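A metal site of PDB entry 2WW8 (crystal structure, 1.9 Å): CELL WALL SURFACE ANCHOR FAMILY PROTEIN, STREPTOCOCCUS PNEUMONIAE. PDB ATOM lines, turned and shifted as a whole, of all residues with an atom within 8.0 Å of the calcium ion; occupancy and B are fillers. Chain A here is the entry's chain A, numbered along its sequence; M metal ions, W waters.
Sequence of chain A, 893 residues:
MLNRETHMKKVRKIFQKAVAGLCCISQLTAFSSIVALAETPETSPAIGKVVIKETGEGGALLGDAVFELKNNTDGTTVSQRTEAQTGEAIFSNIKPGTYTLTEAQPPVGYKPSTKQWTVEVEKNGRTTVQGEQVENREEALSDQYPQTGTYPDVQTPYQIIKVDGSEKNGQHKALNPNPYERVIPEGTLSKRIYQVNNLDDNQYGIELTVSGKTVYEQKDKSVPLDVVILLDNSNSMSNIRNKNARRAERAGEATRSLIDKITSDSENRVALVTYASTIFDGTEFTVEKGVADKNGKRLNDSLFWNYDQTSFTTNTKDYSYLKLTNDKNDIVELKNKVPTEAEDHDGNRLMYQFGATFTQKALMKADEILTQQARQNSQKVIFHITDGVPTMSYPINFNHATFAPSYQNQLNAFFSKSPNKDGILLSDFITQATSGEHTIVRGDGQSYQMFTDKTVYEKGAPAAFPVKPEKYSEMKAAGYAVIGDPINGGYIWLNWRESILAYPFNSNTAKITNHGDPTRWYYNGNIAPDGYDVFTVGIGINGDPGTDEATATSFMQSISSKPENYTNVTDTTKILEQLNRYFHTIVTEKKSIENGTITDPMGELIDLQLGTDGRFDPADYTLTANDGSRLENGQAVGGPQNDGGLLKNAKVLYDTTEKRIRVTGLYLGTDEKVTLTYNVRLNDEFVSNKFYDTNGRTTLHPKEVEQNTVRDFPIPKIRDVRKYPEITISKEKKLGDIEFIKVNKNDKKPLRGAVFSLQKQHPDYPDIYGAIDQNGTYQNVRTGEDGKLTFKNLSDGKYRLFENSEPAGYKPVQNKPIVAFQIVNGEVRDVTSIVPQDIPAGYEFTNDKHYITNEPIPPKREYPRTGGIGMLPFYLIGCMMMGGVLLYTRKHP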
ATOM      1  N   GLN A 609     -24.330  -3.901 -20.377  1.00  0.00           N
ATOM      2  CA  GLN A 609     -23.033  -4.188 -19.733  1.00  0.00           C
ATOM      3  C   GLN A 609     -22.099  -3.068 -20.108  1.00  0.00           C
ATOM      4  O   GLN A 609     -21.785  -2.849 -21.280  1.00  0.00           O
ATOM      5  CB  GLN A 609     -22.445  -5.516 -20.168  1.00  0.00           C
ATOM      6  CG  GLN A 609     -23.376  -6.640 -19.707  1.00  0.00           C
ATOM      7  CD  GLN A 609     -23.536  -6.627 -18.204  1.00  0.00           C
ATOM      8  OE1 GLN A 609     -24.444  -5.995 -17.628  1.00  0.00           O
ATOM      9  NE2 GLN A 609     -22.621  -7.338 -17.538  1.00  0.00           N
ATOM     10  N   LEU A 610     -21.716  -2.296 -19.100  1.00  0.00           N
ATOM     11  CA  LEU A 610     -20.750  -1.211 -19.266  1.00  0.00           C
ATOM     12  C   LEU A 610     -19.363  -1.615 -18.729  1.00  0.00           C
ATOM     13  O   LEU A 610     -18.466  -0.771 -18.606  1.00  0.00           O
ATOM     14  CB  LEU A 610     -21.244   0.027 -18.500  1.00  0.00           C
ATOM     15  CG  LEU A 610     -22.637   0.448 -18.967  1.00  0.00           C
ATOM     16  CD1 LEU A 610     -23.229   1.614 -18.164  1.00  0.00           C
ATOM     17  CD2 LEU A 610     -22.551   0.772 -20.436  1.00  0.00           C
ATOM     18  N   GLY A 611     -19.201  -2.898 -18.385  1.00  0.00           N
ATOM     19  CA  GLY A 611     -18.000  -3.362 -17.676  1.00  0.00           C
ATOM     20  C   GLY A 611     -17.626  -2.599 -16.418  1.00  0.00           C
ATOM     21  O   GLY A 611     -18.349  -1.708 -15.939  1.00  0.00           O
ATOM     22  N   THR A 612     -16.487  -2.930 -15.821  1.00  0.00           N
ATOM     23  CA  THR A 612     -16.144  -2.396 -14.490  1.00  0.00           C
ATOM     24  C   THR A 612     -16.135  -0.869 -14.336  1.00  0.00           C
ATOM     25  O   THR A 612     -16.466  -0.376 -13.264  1.00  0.00           O
ATOM     26  CB  THR A 612     -14.842  -3.041 -13.983  1.00  0.00           C
ATOM     27  OG1 THR A 612     -14.978  -4.461 -14.208  1.00  0.00           O
ATOM     28  CG2 THR A 612     -14.623  -2.805 -12.507  1.00  0.00           C
ATOM     29  N   ASP A 613     -15.796  -0.119 -15.404  1.00  0.00           N
ATOM     30  CA  ASP A 613     -15.744   1.342 -15.283  1.00  0.00           C
ATOM     31  C   ASP A 613     -17.130   1.946 -15.068  1.00  0.00           C
ATOM     32  O   ASP A 613     -17.264   3.104 -14.667  1.00  0.00           O
ATOM     33  CB  ASP A 613     -14.959   2.028 -16.428  1.00  0.00           C
ATOM     34  CG  ASP A 613     -15.438   1.582 -17.823  1.00  0.00           C
ATOM     35  OD1 ASP A 613     -15.846   0.425 -17.923  1.00  0.00           O
ATOM     36  OD2 ASP A 613     -15.407   2.348 -18.831  1.00  0.00           O
ATOM     37  N   GLY A 614     -18.174   1.132 -15.283  1.00  0.00           N
ATOM     38  CA  GLY A 614     -19.522   1.669 -15.253  1.00  0.00           C
ATOM     39  C   GLY A 614     -19.766   2.833 -16.194  1.00  0.00           C
ATOM     40  O   GLY A 614     -20.679   3.607 -15.935  1.00  0.00           O
ATOM     41  N   ARG A 615     -18.978   3.009 -17.260  1.00  0.00           N
ATOM     42  CA  ARG A 615     -19.207   4.059 -18.264  1.00  0.00           C
ATOM     43  C   ARG A 615     -19.245   3.386 -19.649  1.00  0.00           C
ATOM     44  O   ARG A 615     -18.377   2.517 -19.960  1.00  0.00           O
ATOM     45  CB  ARG A 615     -18.064   5.076 -18.352  1.00  0.00           C
ATOM     46  CG  ARG A 615     -18.082   6.244 -17.385  1.00  0.00           C
ATOM     47  CD  ARG A 615     -16.950   7.189 -17.809  1.00  0.00           C
ATOM     48  NE  ARG A 615     -16.534   8.124 -16.754  1.00  0.00           N
ATOM     49  CZ  ARG A 615     -17.161   9.272 -16.488  1.00  0.00           C
ATOM     50  NH1 ARG A 615     -18.244   9.587 -17.183  1.00  0.00           N
ATOM     51  NH2 ARG A 615     -16.730  10.078 -15.524  1.00  0.00           N
ATOM     52  N   PHE A 616     -20.206   3.842 -20.452  1.00  0.00           N
ATOM     53  CA  PHE A 616     -20.308   3.425 -21.870  1.00  0.00           C
ATOM     54  C   PHE A 616     -19.121   3.948 -22.663  1.00  0.00           C
ATOM     55  O   PHE A 616     -18.875   5.152 -22.709  1.00  0.00           O
ATOM     56  CB  PHE A 616     -21.579   3.958 -22.515  1.00  0.00           C
ATOM     57  CG  PHE A 616     -21.868   3.361 -23.869  1.00  0.00           C
ATOM     58  CD1 PHE A 616     -22.301   2.045 -23.993  1.00  0.00           C
ATOM     59  CD2 PHE A 616     -21.697   4.128 -25.011  1.00  0.00           C
ATOM     60  CE1 PHE A 616     -22.552   1.482 -25.234  1.00  0.00           C
ATOM     61  CE2 PHE A 616     -21.977   3.595 -26.259  1.00  0.00           C
ATOM     62  CZ  PHE A 616     -22.409   2.285 -26.375  1.00  0.00           C
ATOM     63  N   ASP A 617     -18.391   3.042 -23.327  1.00  0.00           N
ATOM     64  CA  ASP A 617     -17.189   3.470 -24.019  1.00  0.00           C
ATOM     65  C   ASP A 617     -16.956   2.399 -25.105  1.00  0.00           C
ATOM     66  O   ASP A 617     -17.629   1.363 -25.113  1.00  0.00           O
ATOM     67  CB  ASP A 617     -16.028   3.618 -23.028  1.00  0.00           C
ATOM     68  CG  ASP A 617     -15.298   2.294 -22.813  1.00  0.00           C
ATOM     69  OD1 ASP A 617     -15.938   1.459 -22.123  1.00  0.00           O
ATOM     70  OD2 ASP A 617     -14.179   2.016 -23.343  1.00  0.00           O
ATOM     71  N   PRO A 618     -15.958   2.622 -25.986  1.00  0.00           N
ATOM     72  CA  PRO A 618     -15.775   1.676 -27.095  1.00  0.00           C
ATOM     73  C   PRO A 618     -15.556   0.211 -26.731  1.00  0.00           C
ATOM     74  O   PRO A 618     -15.886  -0.637 -27.567  1.00  0.00           O
ATOM     75  CB  PRO A 618     -14.548   2.265 -27.820  1.00  0.00           C
ATOM     76  CG  PRO A 618     -14.662   3.767 -27.499  1.00  0.00           C
ATOM     77  CD  PRO A 618     -14.952   3.701 -26.030  1.00  0.00           C
ATOM     78  N   ALA A 619     -15.029  -0.101 -25.551  1.00  0.00           N
ATOM     79  CA  ALA A 619     -15.008  -1.494 -25.038  1.00  0.00           C
ATOM     80  C   ALA A 619     -16.375  -2.191 -24.877  1.00  0.00           C
ATOM     81  O   ALA A 619     -16.378  -3.432 -24.730  1.00  0.00           O
ATOM     82  CB  ALA A 619     -14.269  -1.572 -23.698  1.00  0.00           C
ATOM     83  N   ASP A 620     -17.477  -1.448 -24.866  1.00  0.00           N
ATOM     84  CA  ASP A 620     -18.797  -1.992 -24.525  1.00  0.00           C
ATOM     85  C   ASP A 620     -19.657  -2.297 -25.765  1.00  0.00           C
ATOM     86  O   ASP A 620     -20.775  -2.835 -25.634  1.00  0.00           O
ATOM     87  CB  ASP A 620     -19.559  -1.047 -23.611  1.00  0.00           C
ATOM     88  CG  ASP A 620     -18.724  -0.675 -22.430  1.00  0.00           C
ATOM     89  OD1 ASP A 620     -17.975  -1.571 -21.926  1.00  0.00           O
ATOM     90  OD2 ASP A 620     -18.732   0.511 -22.030  1.00  0.00           O
ATOM     91  N   TYR A 621     -19.153  -1.987 -26.945  1.00  0.00           N
ATOM     92  CA  TYR A 621     -19.994  -2.247 -28.119  1.00  0.00           C
ATOM     93  C   TYR A 621     -19.077  -2.470 -29.298  1.00  0.00           C
ATOM     94  O   TYR A 621     -17.893  -2.123 -29.249  1.00  0.00           O
ATOM     95  CB  TYR A 621     -20.947  -1.068 -28.393  1.00  0.00           C
ATOM     96  CG  TYR A 621     -20.202   0.189 -28.851  1.00  0.00           C
ATOM     97  CD1 TYR A 621     -19.957   0.413 -30.223  1.00  0.00           C
ATOM     98  CD2 TYR A 621     -19.718   1.119 -27.920  1.00  0.00           C
ATOM     99  CE1 TYR A 621     -19.246   1.544 -30.637  1.00  0.00           C
ATOM    100  CE2 TYR A 621     -19.036   2.239 -28.318  1.00  0.00           C
ATOM    101  CZ  TYR A 621     -18.814   2.419 -29.683  1.00  0.00           C
ATOM    102  OH  TYR A 621     -18.115   3.524 -30.098  1.00  0.00           O
HETATM  103 CA    CA M   1     -17.109   0.497 -20.252  1.00  0.00          CA
HETATM  104  O   HOH W   1     -15.270  -1.134 -20.187  1.00  0.00           O
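Five residues have an atom within 4 Å of the calcium ion: Leu 610, Asp 613, Arg 615, Asp 617 and Asp 620. The nearest printed residue that does not touch the calcium ion is Gly 611 (4.4 Å).
The side-chain carboxylate (OD2) of Asp 617 lies within hydrogen-bond range of the backbone NH (N) of Ala 619, 3.2 Å away.
The calcium ion is bound by O of Arg 615 (2.4 Å), OD1 of Asp 617 (2.4 Å), OD2 of Asp 620 (2.4 Å), water W1 (2.5 Å), O of Leu 610 (2.5 Å), OD1 of Asp 613 (2.7 Å), OD1 of Asp 620 (2.8 Å) and OD2 of Asp 613 (2.9 Å). The calcium ion has eight donor atoms within binding distance.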
